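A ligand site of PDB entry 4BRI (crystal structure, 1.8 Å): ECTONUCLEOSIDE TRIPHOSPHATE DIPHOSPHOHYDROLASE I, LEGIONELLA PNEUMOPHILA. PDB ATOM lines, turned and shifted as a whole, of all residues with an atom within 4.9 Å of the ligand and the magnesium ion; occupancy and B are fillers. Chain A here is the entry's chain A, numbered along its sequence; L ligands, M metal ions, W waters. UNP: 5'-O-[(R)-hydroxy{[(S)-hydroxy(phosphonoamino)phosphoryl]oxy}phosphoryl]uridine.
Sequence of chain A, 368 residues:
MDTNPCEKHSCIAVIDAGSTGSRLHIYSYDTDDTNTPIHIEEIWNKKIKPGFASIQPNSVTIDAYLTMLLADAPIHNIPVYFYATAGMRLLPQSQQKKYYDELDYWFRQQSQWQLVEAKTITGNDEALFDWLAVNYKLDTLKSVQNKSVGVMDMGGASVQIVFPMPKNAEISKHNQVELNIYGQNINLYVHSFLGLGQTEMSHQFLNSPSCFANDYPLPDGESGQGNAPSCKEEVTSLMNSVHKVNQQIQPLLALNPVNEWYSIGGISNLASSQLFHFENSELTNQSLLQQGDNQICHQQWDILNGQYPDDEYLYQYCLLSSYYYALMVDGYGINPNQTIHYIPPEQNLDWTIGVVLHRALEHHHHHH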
ATOM      1  N   ASP A  16     -19.327 -25.150  22.472  1.00  0.00           N
ATOM      2  CA  ASP A  16     -20.310 -24.052  22.444  1.00  0.00           C
ATOM      3  C   ASP A  16     -19.874 -23.154  21.288  1.00  0.00           C
ATOM      4  O   ASP A  16     -18.868 -22.419  21.429  1.00  0.00           O
ATOM      5  CB  ASP A  16     -20.239 -23.353  23.843  1.00  0.00           C
ATOM      6  CG  ASP A  16     -20.890 -21.964  23.911  1.00  0.00           C
ATOM      7  OD1 ASP A  16     -21.647 -21.564  23.000  1.00  0.00           O
ATOM      8  OD2 ASP A  16     -20.624 -21.261  24.921  1.00  0.00           O
ATOM      9  N   GLY A  18     -20.762 -20.154  20.019  1.00  0.00           N
ATOM     10  CA  GLY A  18     -21.422 -18.873  20.417  1.00  0.00           C
ATOM     11  C   GLY A  18     -21.270 -17.811  19.350  1.00  0.00           C
ATOM     12  O   GLY A  18     -20.473 -17.952  18.351  1.00  0.00           O
ATOM     13  N   SER A  19     -22.023 -16.694  19.498  1.00  0.00           N
ATOM     14  CA  SER A  19     -21.983 -15.643  18.493  1.00  0.00           C
ATOM     15  C   SER A  19     -20.593 -14.934  18.414  1.00  0.00           C
ATOM     16  O   SER A  19     -20.170 -14.516  17.331  1.00  0.00           O
ATOM     17  CB  SER A  19     -23.131 -14.643  18.724  1.00  0.00           C
ATOM     18  OG  SER A  19     -22.815 -13.882  19.870  1.00  0.00           O
ATOM     19  N   THR A  20     -19.893 -14.820  19.523  1.00  0.00           N
ATOM     20  CA  THR A  20     -18.581 -14.129  19.563  1.00  0.00           C
ATOM     21  C   THR A  20     -17.343 -15.043  19.529  1.00  0.00           C
ATOM     22  O   THR A  20     -16.214 -14.570  19.401  1.00  0.00           O
ATOM     23  CB  THR A  20     -18.471 -13.207  20.815  1.00  0.00           C
ATOM     24  OG1 THR A  20     -18.327 -13.991  21.999  1.00  0.00           O
ATOM     25  CG2 THR A  20     -19.702 -12.219  21.012  1.00  0.00           C
ATOM     26  N   GLY A  21     -17.538 -16.354  19.565  1.00  0.00           N
ATOM     27  CA  GLY A  21     -16.375 -17.279  19.639  1.00  0.00           C
ATOM     28  C   GLY A  21     -16.849 -18.713  19.913  1.00  0.00           C
ATOM     29  O   GLY A  21     -18.059 -18.984  20.242  1.00  0.00           O
ATOM     30  N   ARG A  23     -16.090 -22.411  22.056  1.00  0.00           N
ATOM     31  CA  ARG A  23     -15.328 -22.949  23.216  1.00  0.00           C
ATOM     32  C   ARG A  23     -15.469 -24.466  23.241  1.00  0.00           C
ATOM     33  O   ARG A  23     -16.613 -24.996  23.344  1.00  0.00           O
ATOM     34  CB  ARG A  23     -15.886 -22.441  24.547  1.00  0.00           C
ATOM     35  CG  ARG A  23     -15.964 -20.888  24.662  1.00  0.00           C
ATOM     36  CD  ARG A  23     -17.314 -20.417  24.198  1.00  0.00           C
ATOM     37  NE  ARG A  23     -17.220 -19.011  23.829  1.00  0.00           N
ATOM     38  CZ  ARG A  23     -18.273 -18.234  23.524  1.00  0.00           C
ATOM     39  NH1 ARG A  23     -19.529 -18.718  23.647  1.00  0.00           N
ATOM     40  NH2 ARG A  23     -18.074 -16.978  23.174  1.00  0.00           N
ATOM     41  N   LYS A  47     -10.709 -21.696  23.889  1.00  0.00           N
ATOM     42  CA  LYS A  47     -11.640 -20.679  23.309  1.00  0.00           C
ATOM     43  C   LYS A  47     -10.961 -19.992  22.122  1.00  0.00           C
ATOM     44  O   LYS A  47      -9.772 -19.573  22.223  1.00  0.00           O
ATOM     45  CB  LYS A  47     -11.989 -19.621  24.377  1.00  0.00           C
ATOM     46  CG  LYS A  47     -12.416 -20.156  25.729  1.00  0.00           C
ATOM     47  CD  LYS A  47     -13.132 -19.079  26.551  1.00  0.00           C
ATOM     48  CE  LYS A  47     -12.273 -17.822  26.810  1.00  0.00           C
ATOM     49  NZ  LYS A  47     -13.076 -16.724  27.463  1.00  0.00           N
ATOM     50  N   LYS A  49     -11.705 -17.028  18.791  1.00  0.00           N
ATOM     51  CA  LYS A  49     -12.517 -16.021  18.130  1.00  0.00           C
ATOM     52  C   LYS A  49     -12.192 -16.067  16.630  1.00  0.00           C
ATOM     53  O   LYS A  49     -11.117 -16.551  16.263  1.00  0.00           O
ATOM     54  CB  LYS A  49     -12.232 -14.661  18.719  1.00  0.00           C
ATOM     55  CG  LYS A  49     -12.732 -14.549  20.129  1.00  0.00           C
ATOM     56  CD  LYS A  49     -12.380 -13.211  20.738  1.00  0.00           C
ATOM     57  CE  LYS A  49     -12.957 -13.189  22.137  1.00  0.00           C
ATOM     58  NZ  LYS A  49     -12.713 -11.862  22.784  1.00  0.00           N
ATOM     59  N   THR A  85     -25.316 -21.568  18.621  1.00  0.00           N
ATOM     60  CA  THR A  85     -26.375 -20.846  19.261  1.00  0.00           C
ATOM     61  C   THR A  85     -26.798 -19.647  18.429  1.00  0.00           C
ATOM     62  O   THR A  85     -26.956 -19.733  17.197  1.00  0.00           O
ATOM     63  CB  THR A  85     -26.014 -20.478  20.755  1.00  0.00           C
ATOM     64  OG1 THR A  85     -24.749 -19.771  20.806  1.00  0.00           O
ATOM     65  CG2 THR A  85     -25.864 -21.812  21.618  1.00  0.00           C
ATOM     66  N   ALA A  86     -26.962 -18.480  19.043  1.00  0.00           N
ATOM     67  CA  ALA A  86     -27.670 -17.420  18.351  1.00  0.00           C
ATOM     68  C   ALA A  86     -26.978 -16.833  17.125  1.00  0.00           C
ATOM     69  O   ALA A  86     -27.675 -16.315  16.223  1.00  0.00           O
ATOM     70  CB  ALA A  86     -28.023 -16.307  19.360  1.00  0.00           C
ATOM     71  N   GLY A  87     -25.632 -16.845  17.087  1.00  0.00           N
ATOM     72  CA  GLY A  87     -24.990 -16.378  15.822  1.00  0.00           C
ATOM     73  C   GLY A  87     -25.454 -17.157  14.599  1.00  0.00           C
ATOM     74  O   GLY A  87     -25.711 -16.552  13.562  1.00  0.00           O
ATOM     75  N   GLU A 126     -30.998 -24.204  24.578  1.00  0.00           N
ATOM     76  CA  GLU A 126     -29.856 -23.472  25.173  1.00  0.00           C
ATOM     77  C   GLU A 126     -30.198 -23.073  26.632  1.00  0.00           C
ATOM     78  O   GLU A 126     -29.400 -23.283  27.532  1.00  0.00           O
ATOM     79  CB  GLU A 126     -29.604 -22.218  24.348  1.00  0.00           C
ATOM     80  CG  GLU A 126     -28.323 -21.471  24.732  1.00  0.00           C
ATOM     81  CD  GLU A 126     -28.092 -20.317  23.759  1.00  0.00           C
ATOM     82  OE1 GLU A 126     -28.949 -20.085  22.873  1.00  0.00           O
ATOM     83  OE2 GLU A 126     -27.087 -19.610  23.900  1.00  0.00           O
ATOM     84  N   ASP A 153     -28.771 -16.231  31.114  1.00  0.00           N
ATOM     85  CA  ASP A 153     -27.545 -16.237  30.315  1.00  0.00           C
ATOM     86  C   ASP A 153     -27.553 -15.028  29.409  1.00  0.00           C
ATOM     87  O   ASP A 153     -28.430 -14.878  28.588  1.00  0.00           O
ATOM     88  CB  ASP A 153     -27.488 -17.546  29.479  1.00  0.00           C
ATOM     89  CG  ASP A 153     -26.242 -17.703  28.623  1.00  0.00           C
ATOM     90  OD1 ASP A 153     -25.404 -16.755  28.529  1.00  0.00           O
ATOM     91  OD2 ASP A 153     -26.044 -18.848  28.066  1.00  0.00           O
ATOM     92  N   MET A 154     -26.599 -14.112  29.685  1.00  0.00           N
ATOM     93  CA  MET A 154     -26.507 -12.816  29.051  1.00  0.00           C
ATOM     94  C   MET A 154     -25.482 -12.921  27.945  1.00  0.00           C
ATOM     95  O   MET A 154     -24.307 -12.536  28.115  1.00  0.00           O
ATOM     96  CB  MET A 154     -26.049 -11.763  30.125  1.00  0.00           C
ATOM     97  CG  MET A 154     -27.032 -11.622  31.280  1.00  0.00           C
ATOM     98  SD  MET A 154     -28.746 -11.229  30.779  1.00  0.00           S
ATOM     99  CE  MET A 154     -29.447 -10.649  32.367  1.00  0.00           C
ATOM    100  N   GLY A 155     -25.901 -13.410  26.791  1.00  0.00           N
ATOM    101  CA  GLY A 155     -24.929 -13.592  25.668  1.00  0.00           C
ATOM    102  C   GLY A 155     -24.830 -12.415  24.684  1.00  0.00           C
ATOM    103  O   GLY A 155     -25.347 -11.281  24.960  1.00  0.00           O
ATOM    104  N   GLY A 156     -24.169 -12.689  23.569  1.00  0.00           N
ATOM    105  CA  GLY A 156     -23.846 -11.651  22.575  1.00  0.00           C
ATOM    106  C   GLY A 156     -24.950 -11.464  21.552  1.00  0.00           C
ATOM    107  O   GLY A 156     -25.171 -10.313  21.100  1.00  0.00           O
ATOM    108  N   ALA A 157     -25.711 -12.519  21.238  1.00  0.00           N
ATOM    109  CA  ALA A 157     -26.761 -12.348  20.197  1.00  0.00           C
ATOM    110  C   ALA A 157     -28.149 -12.702  20.758  1.00  0.00           C
ATOM    111  O   ALA A 157     -29.173 -12.177  20.235  1.00  0.00           O
ATOM    112  CB  ALA A 157     -26.409 -13.204  18.924  1.00  0.00           C
ATOM    113  N   SER A 158     -28.219 -13.547  21.810  1.00  0.00           N
ATOM    114  CA  SER A 158     -29.503 -13.782  22.459  1.00  0.00           C
ATOM    115  C   SER A 158     -29.263 -13.757  23.992  1.00  0.00           C
ATOM    116  O   SER A 158     -28.078 -13.841  24.455  1.00  0.00           O
ATOM    117  CB  SER A 158     -30.158 -15.104  21.968  1.00  0.00           C
ATOM    118  OG  SER A 158     -29.469 -16.193  22.617  1.00  0.00           O
ATOM    119  N   GLY A 265     -22.602 -15.660  31.286  1.00  0.00           N
ATOM    120  CA  GLY A 265     -22.400 -14.920  30.062  1.00  0.00           C
ATOM    121  C   GLY A 265     -21.591 -13.649  30.250  1.00  0.00           C
ATOM    122  O   GLY A 265     -20.889 -13.430  31.263  1.00  0.00           O
ATOM    123  N   GLY A 266     -21.640 -12.787  29.227  1.00  0.00           N
ATOM    124  CA  GLY A 266     -20.775 -11.619  29.201  1.00  0.00           C
ATOM    125  C   GLY A 266     -21.040 -10.598  30.291  1.00  0.00           C
ATOM    126  O   GLY A 266     -20.179  -9.709  30.566  1.00  0.00           O
ATOM    127  N   SER A 268     -20.623 -11.204  33.367  1.00  0.00           N
ATOM    128  CA  SER A 268     -19.626 -11.395  34.415  1.00  0.00           C
ATOM    129  C   SER A 268     -18.367 -10.567  34.069  1.00  0.00           C
ATOM    130  O   SER A 268     -17.642 -10.131  34.961  1.00  0.00           O
ATOM    131  CB  SER A 268     -19.345 -12.891  34.625  1.00  0.00           C
ATOM    132  OG  SER A 268     -20.528 -13.656  34.983  1.00  0.00           O
ATOM    133  N   ASN A 269     -18.128 -10.338  32.776  1.00  0.00           N
ATOM    134  CA  ASN A 269     -17.025  -9.487  32.318  1.00  0.00           C
ATOM    135  C   ASN A 269     -17.189  -8.039  32.828  1.00  0.00           C
ATOM    136  O   ASN A 269     -16.283  -7.493  33.422  1.00  0.00           O
ATOM    137  CB  ASN A 269     -16.989  -9.385  30.784  1.00  0.00           C
ATOM    138  CG  ASN A 269     -16.649 -10.684  30.118  1.00  0.00           C
ATOM    139  OD1 ASN A 269     -15.878 -11.458  30.667  1.00  0.00           O
ATOM    140  ND2 ASN A 269     -17.223 -10.909  28.897  1.00  0.00           N
ATOM    141  N   ILE A 343     -21.101 -15.561  38.044  1.00  0.00           N
ATOM    142  CA  ILE A 343     -20.040 -16.552  38.231  1.00  0.00           C
ATOM    143  C   ILE A 343     -18.785 -15.832  37.791  1.00  0.00           C
ATOM    144  O   ILE A 343     -18.800 -15.198  36.727  1.00  0.00           O
ATOM    145  CB  ILE A 343     -20.307 -17.770  37.292  1.00  0.00           C
ATOM    146  CG1 ILE A 343     -21.700 -18.406  37.526  1.00  0.00           C
ATOM    147  CG2 ILE A 343     -19.128 -18.780  37.410  1.00  0.00           C
ATOM    148  CD1 ILE A 343     -21.944 -19.058  38.883  1.00  0.00           C
ATOM    149  N   PRO A 344     -17.682 -15.881  38.582  1.00  0.00           N
ATOM    150  CA  PRO A 344     -16.474 -15.145  38.154  1.00  0.00           C
ATOM    151  C   PRO A 344     -16.006 -15.540  36.713  1.00  0.00           C
ATOM    152  O   PRO A 344     -16.060 -16.725  36.387  1.00  0.00           O
ATOM    153  CB  PRO A 344     -15.425 -15.529  39.215  1.00  0.00           C
ATOM    154  CG  PRO A 344     -16.220 -15.915  40.409  1.00  0.00           C
ATOM    155  CD  PRO A 344     -17.546 -16.443  39.938  1.00  0.00           C
ATOM    156  N   PRO A 345     -15.578 -14.552  35.866  1.00  0.00           N
ATOM    157  CA  PRO A 345     -15.367 -14.785  34.419  1.00  0.00           C
ATOM    158  C   PRO A 345     -14.182 -15.696  34.072  1.00  0.00           C
ATOM    159  O   PRO A 345     -14.231 -16.418  33.053  1.00  0.00           O
ATOM    160  CB  PRO A 345     -15.174 -13.363  33.843  1.00  0.00           C
ATOM    161  CG  PRO A 345     -14.732 -12.534  35.018  1.00  0.00           C
ATOM    162  CD  PRO A 345     -15.402 -13.135  36.237  1.00  0.00           C
ATOM    163  N   ASN A 348     -14.979 -19.216  33.056  1.00  0.00           N
ATOM    164  CA  ASN A 348     -15.442 -19.537  31.697  1.00  0.00           C
ATOM    165  C   ASN A 348     -16.662 -20.478  31.667  1.00  0.00           C
ATOM    166  O   ASN A 348     -16.770 -21.345  30.788  1.00  0.00           O
ATOM    167  CB  ASN A 348     -14.295 -20.108  30.875  1.00  0.00           C
ATOM    168  CG  ASN A 348     -13.286 -19.056  30.460  1.00  0.00           C
ATOM    169  OD1 ASN A 348     -12.075 -19.288  30.551  1.00  0.00           O
ATOM    170  ND2 ASN A 348     -13.766 -17.899  29.980  1.00  0.00           N
ATOM    171  N   LEU A 349     -17.561 -20.328  32.643  1.00  0.00           N
ATOM    172  CA  LEU A 349     -18.694 -21.261  32.783  1.00  0.00           C
ATOM    173  C   LEU A 349     -19.730 -20.920  31.748  1.00  0.00           C
ATOM    174  O   LEU A 349     -20.213 -19.799  31.720  1.00  0.00           O
ATOM    175  CB  LEU A 349     -19.355 -21.139  34.171  1.00  0.00           C
ATOM    176  CG  LEU A 349     -20.542 -22.090  34.425  1.00  0.00           C
ATOM    177  CD1 LEU A 349     -20.021 -23.523  34.471  1.00  0.00           C
ATOM    178  CD2 LEU A 349     -21.267 -21.734  35.707  1.00  0.00           C
ATOM    179  N   TRP A 351     -23.010 -23.232  29.134  1.00  0.00           N
ATOM    180  CA  TRP A 351     -24.110 -24.186  29.331  1.00  0.00           C
ATOM    181  C   TRP A 351     -23.703 -25.665  29.037  1.00  0.00           C
ATOM    182  O   TRP A 351     -24.560 -26.585  29.088  1.00  0.00           O
ATOM    183  CB  TRP A 351     -25.308 -23.761  28.470  1.00  0.00           C
ATOM    184  CG  TRP A 351     -24.839 -23.342  27.027  1.00  0.00           C
ATOM    185  CD1 TRP A 351     -24.701 -22.059  26.554  1.00  0.00           C
ATOM    186  CD2 TRP A 351     -24.545 -24.230  25.917  1.00  0.00           C
ATOM    187  NE1 TRP A 351     -24.325 -22.102  25.232  1.00  0.00           N
ATOM    188  CE2 TRP A 351     -24.191 -23.414  24.811  1.00  0.00           C
ATOM    189  CE3 TRP A 351     -24.531 -25.640  25.768  1.00  0.00           C
ATOM    190  CZ2 TRP A 351     -23.790 -23.938  23.583  1.00  0.00           C
ATOM    191  CZ3 TRP A 351     -24.141 -26.192  24.531  1.00  0.00           C
ATOM    192  CH2 TRP A 351     -23.775 -25.334  23.433  1.00  0.00           C
HETATM  193  O2G UNP L   1     -25.556 -15.107  22.005  1.00  0.00           O
HETATM  194  PG  UNP L   1     -24.480 -16.160  22.314  1.00  0.00           P
HETATM  195  O3G UNP L   1     -24.551 -16.923  23.614  1.00  0.00           O
HETATM  196  O1G UNP L   1     -24.322 -17.039  21.070  1.00  0.00           O
HETATM  197  N2B UNP L   1     -23.061 -15.294  22.374  1.00  0.00           N
HETATM  198  PB  UNP L   1     -21.646 -15.668  23.225  1.00  0.00           P
HETATM  199  O1B UNP L   1     -20.495 -15.477  22.299  1.00  0.00           O
HETATM  200  O3B UNP L   1     -21.785 -16.961  24.018  1.00  0.00           O
HETATM  201  O3A UNP L   1     -21.542 -14.396  24.232  1.00  0.00           O
HETATM  202  PA  UNP L   1     -20.913 -14.267  25.731  1.00  0.00           P
HETATM  203  O1A UNP L   1     -21.033 -12.779  26.171  1.00  0.00           O
HETATM  204  O2A UNP L   1     -21.441 -15.100  26.831  1.00  0.00           O
HETATM  205  O5' UNP L   1     -19.380 -14.426  25.543  1.00  0.00           O
HETATM  206  C5' UNP L   1     -18.862 -13.047  25.390  1.00  0.00           C
HETATM  207  C4' UNP L   1     -17.332 -13.032  25.527  1.00  0.00           C
HETATM  208  C3' UNP L   1     -16.711 -14.294  24.907  1.00  0.00           C
HETATM  209  O3' UNP L   1     -15.394 -13.952  24.404  1.00  0.00           O
HETATM  210  C2' UNP L   1     -16.660 -15.246  26.109  1.00  0.00           C
HETATM  211  O2' UNP L   1     -15.746 -16.379  26.077  1.00  0.00           O
HETATM  212  O4' UNP L   1     -16.980 -13.025  26.933  1.00  0.00           O
HETATM  213  C1' UNP L   1     -16.366 -14.286  27.282  1.00  0.00           C
HETATM  214  N1  UNP L   1     -16.816 -14.814  28.586  1.00  0.00           N
HETATM  215  C2  UNP L   1     -15.826 -15.104  29.619  1.00  0.00           C
HETATM  216  O2  UNP L   1     -14.595 -14.888  29.457  1.00  0.00           O
HETATM  217  C6  UNP L   1     -18.138 -15.033  28.840  1.00  0.00           C
HETATM  218  C5  UNP L   1     -18.485 -15.543  30.101  1.00  0.00           C
HETATM  219  C4  UNP L   1     -17.496 -15.820  31.093  1.00  0.00           C
HETATM  220  N3  UNP L   1     -16.194 -15.586  30.820  1.00  0.00           N
HETATM  221  O4  UNP L   1     -17.789 -16.275  32.252  1.00  0.00           O
HETATM  222 MG    MG M   1     -23.428 -18.014  24.754  1.00  0.00          MG
HETATM  223  O   HOH W   1     -20.008 -17.600  26.987  1.00  0.00           O
HETATM  224  O   HOH W   2     -23.339 -19.615  23.409  1.00  0.00           O
HETATM  225  O   HOH W   3     -25.004 -18.996  25.586  1.00  0.00           O
HETATM  226  O   HOH W   4     -20.352 -16.743  32.861  1.00  0.00           O
HETATM  227  O   HOH W   5     -22.014 -19.189  25.940  1.00  0.00           O
HETATM  228  O   HOH W   6     -17.661 -18.034  34.447  1.00  0.00           O
HETATM  229  O   HOH W   7     -18.830 -10.039  26.923  1.00  0.00           O
HETATM  230  O   HOH W   8     -17.269 -18.340  27.233  1.00  0.00           O
HETATM  231  O   HOH W   9     -26.896 -16.363  25.139  1.00  0.00           O
HETATM  232  O   HOH W  10     -23.540 -16.790  26.399  1.00  0.00           O
HETATM  233  O   HOH W  11     -27.178 -17.764  21.963  1.00  0.00           O
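The backbone NH (N) of Thr 20 lies within hydrogen-bond range of an oxygen (O1B) of the ligand (2.9 Å). O1B of the ligand is in hydrogen-bond range of OG1 of Thr 20 (2.6 Å). The backbone NH of Ala 157 sits at hydrogen-bond distance from an oxygen (O2G) of the ligand (2.7 Å). The side-chain hydroxyl (OG1) of Thr 85 is in hydrogen-bond range of an oxygen (O1G) of the ligand (2.8 Å). The backbone NH (N) of Ser 19 sits at hydrogen-bond distance from an oxygen (O1G) of the ligand (2.8 Å). The side-chain hydroxyl (OG) of Ser 19 sits at hydrogen-bond distance from a nitrogen (N2B) of the ligand (2.9 Å). NH2 of Arg 23 is in salt-bridge range of O1B of the ligand (3.0 Å). An oxygen (O4') of the ligand lies within hydrogen-bond range of the side-chain amide nitrogen (ND2) of Asn 269, 2.9 Å away. The side-chain amino group of Lys 47 lies within hydrogen-bond range of an oxygen (O2') of the ligand. N of Gly 156 sits at hydrogen-bond distance from O2G of the ligand, 3.2 Å away. The backbone carbonyl oxygen of Pro 345 is in hydrogen-bond range of a nitrogen (N3) of the ligand, 3.1 Å away. O2G of the ligand is in hydrogen-bond range of N of Ser 158, at 3.1 Å. N of Gly 266 is in hydrogen-bond range of O1A of the ligand, 3.1 Å away. ND2 of Asn 348 lies within hydrogen-bond range of O2 of the ligand, at 3.2 Å.
The guanidinium group of Arg 23 is in hydrogen-bond range of the side-chain hydroxyl of Thr 20 (3.2 Å). The side-chain hydroxyl of Ser 19 is in hydrogen-bond range of the backbone NH of Ala 157. NH1 of Arg 23 lies within salt-bridge range of OD2 of Asp 16 (3.0 Å). ND2 of Asn 348 sits close to NZ of Lys 47, at 2.9 Å. The backbone carbonyl oxygen (O) of Pro 345 sits at hydrogen-bond distance from the side-chain amide nitrogen (ND2) of Asn 348. N of Gly 266 sits at hydrogen-bond distance from O of Met 154 (2.9 Å). N of Gly 18 sits close to OD1 of Asp 16 (3.4 Å).
Gly 18 touches the ligand (CA to O1G, 3.5 Å). CE of Lys 49 touches O3' of the ligand, at 3.4 Å. Ala 86 touches the ligand (N to O1G, 3.6 Å). Glu 126 touches the ligand (OE2 to O3G, 3.7 Å). Met 154 touches the ligand. Gly 155 touches the ligand (CA to O3A, 3.8 Å). Gly 265 touches the ligand. Of the 28 residues printed, 19 come within 4 Å of the ligand. The nearest printed residue that does not touch the ligand is Leu 349 (4.1 Å).
No residue comes within 4 Å of the magnesium ion. The nearest printed residue that does not touch the magnesium ion is Glu 126 (4.1 Å).
The magnesium ion is bound by O3G of the ligand (1.9 Å), water W3 (2.0 Å), water W10 (2.1 Å), O3B of the ligand (2.1 Å), water W2 (2.1 Å) and water W5 (2.2 Å).
Water W5 lies within hydrogen-bond range of OD2 of Asp 16 (2.7 Å) and NH1 of Arg 23 (3.4 Å). Water W2 lies within hydrogen-bond range of OD1 of Asp 16 (2.6 Å), OG1 of Thr 85 (3.0 Å) and NE1 of Trp 351 (3.2 Å). Water W10 bridges an oxygen (O2A) of the ligand (2.7 Å) and the side-chain carboxylate of Asp 153 (2.8 Å). Water W8 bridges O2' of the ligand and NE of Arg 23. Water W9 bridges the backbone carbonyl oxygen of Ser 158 (2.9 Å) and the side-chain carboxylate of Glu 126 (3.5 Å). Water W11 lies within hydrogen-bond range of the side-chain carboxylate (OE2) of Glu 126, the side-chain hydroxyl (OG) of Ser 158, the backbone NH (N) of Ala 86, an oxygen (O1G) of the ligand and the side-chain hydroxyl (OG1) of Thr 85.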
